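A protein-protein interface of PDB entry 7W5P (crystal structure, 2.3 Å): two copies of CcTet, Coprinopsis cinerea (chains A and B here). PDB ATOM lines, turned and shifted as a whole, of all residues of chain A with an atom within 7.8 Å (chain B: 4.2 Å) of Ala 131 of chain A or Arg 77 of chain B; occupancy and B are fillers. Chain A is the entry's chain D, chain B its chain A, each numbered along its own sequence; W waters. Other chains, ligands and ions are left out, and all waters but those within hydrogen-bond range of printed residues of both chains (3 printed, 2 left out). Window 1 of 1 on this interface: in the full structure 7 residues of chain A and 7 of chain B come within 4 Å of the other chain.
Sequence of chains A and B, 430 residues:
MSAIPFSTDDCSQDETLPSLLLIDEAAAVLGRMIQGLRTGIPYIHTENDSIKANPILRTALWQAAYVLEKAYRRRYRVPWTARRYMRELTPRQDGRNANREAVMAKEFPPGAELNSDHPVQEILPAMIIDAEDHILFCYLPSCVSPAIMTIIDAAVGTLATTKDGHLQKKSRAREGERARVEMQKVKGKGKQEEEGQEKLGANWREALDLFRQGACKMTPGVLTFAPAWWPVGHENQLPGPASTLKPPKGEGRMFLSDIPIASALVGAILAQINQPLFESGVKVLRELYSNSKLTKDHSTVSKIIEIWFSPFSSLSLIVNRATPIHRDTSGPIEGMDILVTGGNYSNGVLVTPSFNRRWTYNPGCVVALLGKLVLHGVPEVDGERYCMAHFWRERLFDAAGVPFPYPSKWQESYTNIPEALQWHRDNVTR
Hydrophobic or aromatic side chains of chain A that line the printed part of chain B: Pro 79 and Ala 131. Among the printed residues, 9 pairs touch across the chains.
Ala 131 of chain A touches just these residues of chain B: Arg 77, Pro 79 and Ala 131. Printed residues of chain A within 4 Å of Arg 77 of chain B: Pro 79 (3.6 Å) and Ala 131 (3.7 Å). Of the printed residues of chain B, Thr 81 of chain A touches Ala 131. Of the printed residues of chain B, Pro 79 of chain A touches Arg 77 and Asp 133. Of the printed residues of chain A, Ala 131 of chain B touches Thr 81 (3.7 Å), Ala 131 (3.5 Å) and Glu 132 (3.6 Å). Printed residues of chain B within 4 Å of Asp 133 of chain A: Pro 79. Of the printed residues of chain A, Pro 79 of chain B touches Ala 131, Glu 132 and Asp 133. The nearest residue of chain B that does not touch Ala 131 of chain A is Val 78 of chain B (4.1 Å). The nearest residue of chain A that does not touch Arg 77 of chain B is Arg 77 of chain A (4.6 Å).
The backbone NH (N) of Arg 77 of chain B lies within hydrogen-bond range of the side-chain carboxylate (OE1) of Glu 113 of chain B (3.1 Å). The guanidinium group of Arg 77 of chain B lies within hydrogen-bond range of the backbone carbonyl oxygen of Asp 130 of chain B. OD1 of Asp 133 of chain B is in salt-bridge range of NH1 of Arg 77 of chain B (3.0 Å). The side-chain carboxylate of Asp 133 of chain A is in salt-bridge range of the guanidinium group of Arg 77 of chain A, 3.0 Å away. O of Trp 80 of chain A lies within hydrogen-bond range of N of Ala 131 of chain A. The guanidinium group (NH1) of Arg 83 of chain A is in salt-bridge range of the side-chain carboxylate (OE1) of Glu 132 of chain A.
Pro 79 of chain A touches Arg 77 of chain B, but with the chains exchanged Arg 77 of chain A does not touch Pro 79 of chain B (4.8 Å). Pro 79 of chain A touches Asp 133 of chain B, and with the chains exchanged Asp 133 of chain A touches Pro 79 of chain B. Ala 131 of chain A touches Arg 77 of chain B, but with the chains exchanged Arg 77 of chain A does not touch Ala 131 of chain B (7.3 Å). Ala 131 of chain A touches Pro 79 of chain B, but with the chains exchanged Pro 79 of chain A does not touch Ala 131 of chain B (5.1 Å). Positions printed for both chains: 76, 77, 78, 79, 113, 129, 130, 131 and 133. Of the 9 pairs that touch across the chains among the printed residues, 3 have their exchanged pair printed and touching as well.
Water W2 lies within hydrogen-bond range of NE of Arg 77 of chain A (2.6 Å), OE2 of Glu 113 of chain A (3.0 Å) and OE2 of Glu 113 of chain B (3.2 Å). Water W1 lies within hydrogen-bond range of O of Pro 79 of chain A (2.7 Å) and OD2 of Asp 133 of chain B (2.9 Å). Water W3 lies within hydrogen-bond range of O of Pro 79 of chain B (2.8 Å) and NZ of Lys 409 of chain A (3.0 Å).
NH2 of Arg 77 of chain B touches CB of Pro 79 of chain A (3.6 Å). Asp 133 of chain B touches Pro 79 of chain A. CG2 of Thr 81 of chain A touches O of Ala 131 of chain B, at 3.7 Å. Arg 77 of chain B touches Ala 131 of chain A (CD to CB, 3.7 Å). Pro 79 of chain B touches Ala 131 of chain A. CB of Ala 131 of chain A touches O of Ala 131 of chain B (3.5 Å). CA of Glu 132 of chain A touches O of Pro 79 of chain B (3.8 Å). Glu 132 of chain A touches Ala 131 of chain B (CG to CB, 3.6 Å). Asp 133 of chain A touches Pro 79 of chain B (OD2 to CB, 3.2 Å).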
ATOM      1  N   TYR A  76      15.412  30.876  10.154  1.00  0.00           N
ATOM      2  CA  TYR A  76      14.829  31.656  11.234  1.00  0.00           C
ATOM      3  C   TYR A  76      15.000  30.926  12.559  1.00  0.00           C
ATOM      4  O   TYR A  76      14.883  29.701  12.629  1.00  0.00           O
ATOM      5  CB  TYR A  76      13.345  31.904  10.985  1.00  0.00           C
ATOM      6  CG  TYR A  76      13.050  32.695   9.738  1.00  0.00           C
ATOM      7  CD1 TYR A  76      12.982  34.084   9.776  1.00  0.00           C
ATOM      8  CD2 TYR A  76      12.839  32.059   8.523  1.00  0.00           C
ATOM      9  CE1 TYR A  76      12.708  34.815   8.644  1.00  0.00           C
ATOM     10  CE2 TYR A  76      12.564  32.782   7.381  1.00  0.00           C
ATOM     11  CZ  TYR A  76      12.499  34.161   7.449  1.00  0.00           C
ATOM     12  OH  TYR A  76      12.223  34.891   6.315  1.00  0.00           O
ATOM     13  N   ARG A  77      15.166  31.698  13.629  1.00  0.00           N
ATOM     14  CA  ARG A  77      15.387  31.152  14.959  1.00  0.00           C
ATOM     15  C   ARG A  77      14.305  31.659  15.897  1.00  0.00           C
ATOM     16  O   ARG A  77      14.016  32.861  15.926  1.00  0.00           O
ATOM     17  CB  ARG A  77      16.773  31.538  15.487  1.00  0.00           C
ATOM     18  CG  ARG A  77      17.140  30.881  16.813  1.00  0.00           C
ATOM     19  CD  ARG A  77      18.459  31.416  17.365  1.00  0.00           C
ATOM     20  NE  ARG A  77      19.580  31.170  16.459  1.00  0.00           N
ATOM     21  CZ  ARG A  77      20.313  30.059  16.458  1.00  0.00           C
ATOM     22  NH1 ARG A  77      20.044  29.081  17.317  1.00  0.00           N
ATOM     23  NH2 ARG A  77      21.315  29.922  15.595  1.00  0.00           N
ATOM     24  N   VAL A  78      13.700  30.746  16.653  1.00  0.00           N
ATOM     25  CA  VAL A  78      12.749  31.138  17.691  1.00  0.00           C
ATOM     26  C   VAL A  78      13.542  31.373  18.970  1.00  0.00           C
ATOM     27  O   VAL A  78      14.582  30.726  19.178  1.00  0.00           O
ATOM     28  CB  VAL A  78      11.658  30.074  17.905  1.00  0.00           C
ATOM     29  CG1 VAL A  78      10.695  30.034  16.715  1.00  0.00           C
ATOM     30  CG2 VAL A  78      12.290  28.707  18.166  1.00  0.00           C
ATOM     31  N   PRO A  79      13.097  32.265  19.852  1.00  0.00           N
ATOM     32  CA  PRO A  79      13.902  32.595  21.035  1.00  0.00           C
ATOM     33  C   PRO A  79      13.701  31.626  22.189  1.00  0.00           C
ATOM     34  O   PRO A  79      13.647  32.052  23.349  1.00  0.00           O
ATOM     35  CB  PRO A  79      13.405  33.997  21.404  1.00  0.00           C
ATOM     36  CG  PRO A  79      11.962  33.980  21.003  1.00  0.00           C
ATOM     37  CD  PRO A  79      11.887  33.103  19.757  1.00  0.00           C
ATOM     38  N   TRP A  80      13.565  30.335  21.889  1.00  0.00           N
ATOM     39  CA  TRP A  80      13.416  29.314  22.920  1.00  0.00           C
ATOM     40  C   TRP A  80      13.886  27.978  22.356  1.00  0.00           C
ATOM     41  O   TRP A  80      14.145  27.842  21.158  1.00  0.00           O
ATOM     42  CB  TRP A  80      11.973  29.228  23.425  1.00  0.00           C
ATOM     43  CG  TRP A  80      10.949  29.464  22.352  1.00  0.00           C
ATOM     44  CD1 TRP A  80      10.323  30.646  22.052  1.00  0.00           C
ATOM     45  CD2 TRP A  80      10.436  28.495  21.433  1.00  0.00           C
ATOM     46  NE1 TRP A  80       9.450  30.465  21.004  1.00  0.00           N
ATOM     47  CE2 TRP A  80       9.501  29.154  20.606  1.00  0.00           C
ATOM     48  CE3 TRP A  80      10.676  27.131  21.227  1.00  0.00           C
ATOM     49  CZ2 TRP A  80       8.809  28.494  19.593  1.00  0.00           C
ATOM     50  CZ3 TRP A  80       9.986  26.478  20.221  1.00  0.00           C
ATOM     51  CH2 TRP A  80       9.062  27.161  19.418  1.00  0.00           C
ATOM     52  N   THR A  81      14.039  27.007  23.245  1.00  0.00           N
ATOM     53  CA  THR A  81      14.446  25.663  22.863  1.00  0.00           C
ATOM     54  C   THR A  81      13.232  24.751  22.752  1.00  0.00           C
ATOM     55  O   THR A  81      12.250  24.901  23.488  1.00  0.00           O
ATOM     56  CB  THR A  81      15.424  25.066  23.875  1.00  0.00           C
ATOM     57  OG1 THR A  81      14.766  24.935  25.139  1.00  0.00           O
ATOM     58  CG2 THR A  81      16.656  25.944  24.021  1.00  0.00           C
ATOM     59  N   ALA A  82      13.317  23.787  21.831  1.00  0.00           N
ATOM     60  CA  ALA A  82      12.274  22.769  21.736  1.00  0.00           C
ATOM     61  C   ALA A  82      12.102  22.026  23.054  1.00  0.00           C
ATOM     62  O   ALA A  82      10.989  21.612  23.389  1.00  0.00           O
ATOM     63  CB  ALA A  82      12.591  21.775  20.613  1.00  0.00           C
ATOM     64  N   ARG A  83      13.185  21.864  23.820  1.00  0.00           N
ATOM     65  CA  ARG A  83      13.112  21.119  25.076  1.00  0.00           C
ATOM     66  C   ARG A  83      12.204  21.821  26.085  1.00  0.00           C
ATOM     67  O   ARG A  83      11.335  21.191  26.702  1.00  0.00           O
ATOM     68  CB  ARG A  83      14.525  20.934  25.643  1.00  0.00           C
ATOM     69  CG  ARG A  83      14.610  20.140  26.946  1.00  0.00           C
ATOM     70  CD  ARG A  83      15.895  20.461  27.726  1.00  0.00           C
ATOM     71  NE  ARG A  83      16.173  21.897  27.787  1.00  0.00           N
ATOM     72  CZ  ARG A  83      17.240  22.480  27.243  1.00  0.00           C
ATOM     73  NH1 ARG A  83      18.139  21.750  26.594  1.00  0.00           N
ATOM     74  NH2 ARG A  83      17.409  23.793  27.347  1.00  0.00           N
ATOM     75  N   GLY A 111       9.378  35.576  18.293  1.00  0.00           N
ATOM     76  CA  GLY A 111      10.675  36.208  18.383  1.00  0.00           C
ATOM     77  C   GLY A 111      10.879  37.259  17.309  1.00  0.00           C
ATOM     78  O   GLY A 111      10.140  37.352  16.329  1.00  0.00           O
ATOM     79  N   GLU A 113      13.120  37.734  14.902  1.00  0.00           N
ATOM     80  CA  GLU A 113      13.377  37.272  13.512  1.00  0.00           C
ATOM     81  C   GLU A 113      12.116  36.862  12.759  1.00  0.00           C
ATOM     82  O   GLU A 113      12.080  36.994  11.590  1.00  0.00           O
ATOM     83  CB  GLU A 113      14.316  36.077  13.421  1.00  0.00           C
ATOM     84  CG  GLU A 113      15.577  36.224  14.204  1.00  0.00           C
ATOM     85  CD  GLU A 113      16.646  35.216  13.894  1.00  0.00           C
ATOM     86  OE1 GLU A 113      16.446  34.396  13.095  1.00  0.00           O
ATOM     87  OE2 GLU A 113      17.653  35.293  14.479  1.00  0.00           O
ATOM     88  N   ILE A 129      14.752  26.996  13.343  1.00  0.00           N
ATOM     89  CA  ILE A 129      15.576  26.309  14.323  1.00  0.00           C
ATOM     90  C   ILE A 129      15.321  26.945  15.683  1.00  0.00           C
ATOM     91  O   ILE A 129      14.874  28.092  15.783  1.00  0.00           O
ATOM     92  CB  ILE A 129      17.069  26.361  13.953  1.00  0.00           C
ATOM     93  CG1 ILE A 129      17.571  27.807  13.972  1.00  0.00           C
ATOM     94  CG2 ILE A 129      17.294  25.741  12.575  1.00  0.00           C
ATOM     95  CD1 ILE A 129      19.022  27.966  13.515  1.00  0.00           C
ATOM     96  N   ASP A 130      15.602  26.184  16.739  1.00  0.00           N
ATOM     97  CA  ASP A 130      15.391  26.689  18.084  1.00  0.00           C
ATOM     98  C   ASP A 130      16.672  27.345  18.605  1.00  0.00           C
ATOM     99  O   ASP A 130      17.678  27.456  17.898  1.00  0.00           O
ATOM    100  CB  ASP A 130      14.882  25.574  19.005  1.00  0.00           C
ATOM    101  CG  ASP A 130      15.953  24.559  19.377  1.00  0.00           C
ATOM    102  OD1 ASP A 130      17.048  24.553  18.771  1.00  0.00           O
ATOM    103  OD2 ASP A 130      15.684  23.747  20.288  1.00  0.00           O
ATOM    104  N   ALA A 131      16.638  27.778  19.868  1.00  0.00           N
ATOM    105  CA  ALA A 131      17.773  28.470  20.469  1.00  0.00           C
ATOM    106  C   ALA A 131      19.006  27.586  20.602  1.00  0.00           C
ATOM    107  O   ALA A 131      20.090  28.110  20.858  1.00  0.00           O
ATOM    108  CB  ALA A 131      17.386  29.028  21.841  1.00  0.00           C
ATOM    109  N   GLU A 132      18.876  26.273  20.425  1.00  0.00           N
ATOM    110  CA  GLU A 132      20.009  25.356  20.495  1.00  0.00           C
ATOM    111  C   GLU A 132      20.254  24.657  19.165  1.00  0.00           C
ATOM    112  O   GLU A 132      20.779  23.541  19.138  1.00  0.00           O
ATOM    113  CB  GLU A 132      19.802  24.311  21.589  1.00  0.00           C
ATOM    114  CG  GLU A 132      20.013  24.813  22.991  1.00  0.00           C
ATOM    115  CD  GLU A 132      19.629  23.779  24.033  1.00  0.00           C
ATOM    116  OE1 GLU A 132      18.917  22.812  23.683  1.00  0.00           O
ATOM    117  OE2 GLU A 132      20.041  23.934  25.202  1.00  0.00           O
ATOM    118  N   ASP A 133      19.865  25.292  18.056  1.00  0.00           N
ATOM    119  CA  ASP A 133      20.184  24.839  16.703  1.00  0.00           C
ATOM    120  C   ASP A 133      19.477  23.542  16.308  1.00  0.00           C
ATOM    121  O   ASP A 133      19.929  22.850  15.394  1.00  0.00           O
ATOM    122  CB  ASP A 133      21.695  24.686  16.498  1.00  0.00           C
ATOM    123  CG  ASP A 133      22.407  26.019  16.439  1.00  0.00           C
ATOM    124  OD1 ASP A 133      21.804  26.988  15.938  1.00  0.00           O
ATOM    125  OD2 ASP A 133      23.574  26.096  16.866  1.00  0.00           O
ATOM    126  N   HIS A 134      18.416  23.155  17.009  1.00  0.00           N
ATOM    127  CA  HIS A 134      17.609  22.018  16.587  1.00  0.00           C
ATOM    128  C   HIS A 134      16.566  22.464  15.565  1.00  0.00           C
ATOM    129  O   HIS A 134      15.988  23.549  15.681  1.00  0.00           O
ATOM    130  CB  HIS A 134      16.945  21.349  17.790  1.00  0.00           C
ATOM    131  CG  HIS A 134      17.913  20.634  18.681  1.00  0.00           C
ATOM    132  ND1 HIS A 134      18.195  21.054  19.964  1.00  0.00           N
ATOM    133  CD2 HIS A 134      18.686  19.542  18.465  1.00  0.00           C
ATOM    134  CE1 HIS A 134      19.090  20.246  20.504  1.00  0.00           C
ATOM    135  NE2 HIS A 134      19.404  19.321  19.614  1.00  0.00           N
ATOM    136  N   LEU A 136      13.091  22.489  13.734  1.00  0.00           N
ATOM    137  CA  LEU A 136      11.685  22.328  14.125  1.00  0.00           C
ATOM    138  C   LEU A 136      10.778  22.223  12.899  1.00  0.00           C
ATOM    139  O   LEU A 136       9.798  21.637  12.997  1.00  0.00           O
ATOM    140  CB  LEU A 136      11.228  23.477  15.020  1.00  0.00           C
ATOM    141  CG  LEU A 136      12.154  23.963  16.123  1.00  0.00           C
ATOM    142  CD1 LEU A 136      11.607  25.237  16.668  1.00  0.00           C
ATOM    143  CD2 LEU A 136      12.293  22.968  17.221  1.00  0.00           C
ATOM    144  N   LYS A 409      21.525  18.446  15.417  1.00  0.00           N
ATOM    145  CA  LYS A 409      21.624  19.868  15.120  1.00  0.00           C
ATOM    146  C   LYS A 409      21.870  20.072  13.628  1.00  0.00           C
ATOM    147  O   LYS A 409      22.452  19.219  12.951  1.00  0.00           O
ATOM    148  CB  LYS A 409      22.725  20.517  15.963  1.00  0.00           C
ATOM    149  CG  LYS A 409      22.449  20.406  17.460  1.00  0.00           C
ATOM    150  CD  LYS A 409      23.441  21.186  18.306  1.00  0.00           C
ATOM    151  CE  LYS A 409      23.178  20.959  19.792  1.00  0.00           C
ATOM    152  NZ  LYS A 409      23.714  22.056  20.639  1.00  0.00           N
ATOM    153  N   TYR B  76      22.921  39.226  21.604  1.00  0.00           N
ATOM    154  CA  TYR B  76      23.418  38.031  20.938  1.00  0.00           C
ATOM    155  C   TYR B  76      23.106  36.804  21.780  1.00  0.00           C
ATOM    156  O   TYR B  76      23.052  36.871  23.011  1.00  0.00           O
ATOM    157  CB  TYR B  76      24.931  38.094  20.733  1.00  0.00           C
ATOM    158  CG  TYR B  76      25.444  39.145  19.787  1.00  0.00           C
ATOM    159  CD1 TYR B  76      25.538  38.892  18.424  1.00  0.00           C
ATOM    160  CD2 TYR B  76      25.869  40.379  20.260  1.00  0.00           C
ATOM    161  CE1 TYR B  76      26.028  39.846  17.554  1.00  0.00           C
ATOM    162  CE2 TYR B  76      26.363  41.343  19.398  1.00  0.00           C
ATOM    163  CZ  TYR B  76      26.439  41.071  18.046  1.00  0.00           C
ATOM    164  OH  TYR B  76      26.928  42.023  17.181  1.00  0.00           O
ATOM    165  N   ARG B  77      22.921  35.673  21.108  1.00  0.00           N
ATOM    166  CA  ARG B  77      22.621  34.411  21.772  1.00  0.00           C
ATOM    167  C   ARG B  77      23.643  33.361  21.359  1.00  0.00           C
ATOM    168  O   ARG B  77      23.943  33.215  20.169  1.00  0.00           O
ATOM    169  CB  ARG B  77      21.210  33.919  21.436  1.00  0.00           C
ATOM    170  CG  ARG B  77      20.787  32.710  22.276  1.00  0.00           C
ATOM    171  CD  ARG B  77      19.482  32.108  21.794  1.00  0.00           C
ATOM    172  NE  ARG B  77      18.409  33.094  21.772  1.00  0.00           N
ATOM    173  CZ  ARG B  77      17.648  33.394  22.819  1.00  0.00           C
ATOM    174  NH1 ARG B  77      17.839  32.782  23.981  1.00  0.00           N
ATOM    175  NH2 ARG B  77      16.695  34.305  22.703  1.00  0.00           N
ATOM    176  N   VAL B  78      24.192  32.649  22.341  1.00  0.00           N
ATOM    177  CA  VAL B  78      25.037  31.492  22.060  1.00  0.00           C
ATOM    178  C   VAL B  78      24.117  30.275  22.029  1.00  0.00           C
ATOM    179  O   VAL B  78      23.101  30.254  22.740  1.00  0.00           O
ATOM    180  CB  VAL B  78      26.172  31.334  23.089  1.00  0.00           C
ATOM    181  CG1 VAL B  78      27.133  32.527  23.013  1.00  0.00           C
ATOM    182  CG2 VAL B  78      25.619  31.165  24.498  1.00  0.00           C
ATOM    183  N   PRO B  79      24.424  29.246  21.234  1.00  0.00           N
ATOM    184  CA  PRO B  79      23.487  28.124  21.087  1.00  0.00           C
ATOM    185  C   PRO B  79      23.623  27.070  22.175  1.00  0.00           C
ATOM    186  O   PRO B  79      23.519  25.870  21.900  1.00  0.00           O
ATOM    187  CB  PRO B  79      23.862  27.551  19.718  1.00  0.00           C
ATOM    188  CG  PRO B  79      25.347  27.769  19.654  1.00  0.00           C
ATOM    189  CD  PRO B  79      25.594  29.100  20.352  1.00  0.00           C
ATOM    190  N   GLU B 113      25.414  33.615  15.302  1.00  0.00           N
ATOM    191  CA  GLU B 113      25.323  35.057  15.497  1.00  0.00           C
ATOM    192  C   GLU B 113      26.682  35.698  15.758  1.00  0.00           C
ATOM    193  O   GLU B 113      26.834  36.900  15.528  1.00  0.00           O
ATOM    194  CB  GLU B 113      24.377  35.382  16.659  1.00  0.00           C
ATOM    195  CG  GLU B 113      22.985  34.788  16.522  1.00  0.00           C
ATOM    196  CD  GLU B 113      21.989  35.358  17.525  1.00  0.00           C
ATOM    197  OE1 GLU B 113      22.313  36.360  18.198  1.00  0.00           O
ATOM    198  OE2 GLU B 113      20.875  34.800  17.632  1.00  0.00           O
ATOM    199  N   ILE B 129      23.336  36.479  25.692  1.00  0.00           N
ATOM    200  CA  ILE B 129      22.442  35.636  26.471  1.00  0.00           C
ATOM    201  C   ILE B 129      22.618  34.196  26.006  1.00  0.00           C
ATOM    202  O   ILE B 129      23.080  33.927  24.894  1.00  0.00           O
ATOM    203  CB  ILE B 129      20.965  36.075  26.354  1.00  0.00           C
ATOM    204  CG1 ILE B 129      20.501  36.044  24.893  1.00  0.00           C
ATOM    205  CG2 ILE B 129      20.765  37.466  26.936  1.00  0.00           C
ATOM    206  CD1 ILE B 129      19.089  36.575  24.691  1.00  0.00           C
ATOM    207  N   ASP B 130      22.257  33.262  26.880  1.00  0.00           N
ATOM    208  CA  ASP B 130      22.383  31.859  26.532  1.00  0.00           C
ATOM    209  C   ASP B 130      21.077  31.351  25.921  1.00  0.00           C
ATOM    210  O   ASP B 130      20.121  32.106  25.714  1.00  0.00           O
ATOM    211  CB  ASP B 130      22.828  31.046  27.752  1.00  0.00           C
ATOM    212  CG  ASP B 130      21.733  30.867  28.790  1.00  0.00           C
ATOM    213  OD1 ASP B 130      20.651  31.492  28.688  1.00  0.00           O
ATOM    214  OD2 ASP B 130      21.979  30.088  29.735  1.00  0.00           O
ATOM    215  N   ALA B 131      21.029  30.049  25.631  1.00  0.00           N
ATOM    216  CA  ALA B 131      19.850  29.475  24.992  1.00  0.00           C
ATOM    217  C   ALA B 131      18.612  29.525  25.879  1.00  0.00           C
ATOM    218  O   ALA B 131      17.503  29.324  25.369  1.00  0.00           O
ATOM    219  CB  ALA B 131      20.127  28.032  24.565  1.00  0.00           C
ATOM    220  N   ASP B 133      17.948  32.312  27.891  1.00  0.00           N
ATOM    221  CA  ASP B 133      17.745  33.737  28.145  1.00  0.00           C
ATOM    222  C   ASP B 133      18.488  34.251  29.373  1.00  0.00           C
ATOM    223  O   ASP B 133      18.168  35.332  29.876  1.00  0.00           O
ATOM    224  CB  ASP B 133      16.256  34.082  28.262  1.00  0.00           C
ATOM    225  CG  ASP B 133      15.478  33.713  27.015  1.00  0.00           C
ATOM    226  OD1 ASP B 133      15.909  34.101  25.908  1.00  0.00           O
ATOM    227  OD2 ASP B 133      14.439  33.034  27.150  1.00  0.00           O
HETATM  228  O   HOH W   1      12.462  31.462  25.727  1.00  0.00           O
HETATM  229  O   HOH W   2      19.897  33.291  14.973  1.00  0.00           O
HETATM  230  O   HOH W   3      23.176  23.446  23.214  1.00  0.00           O
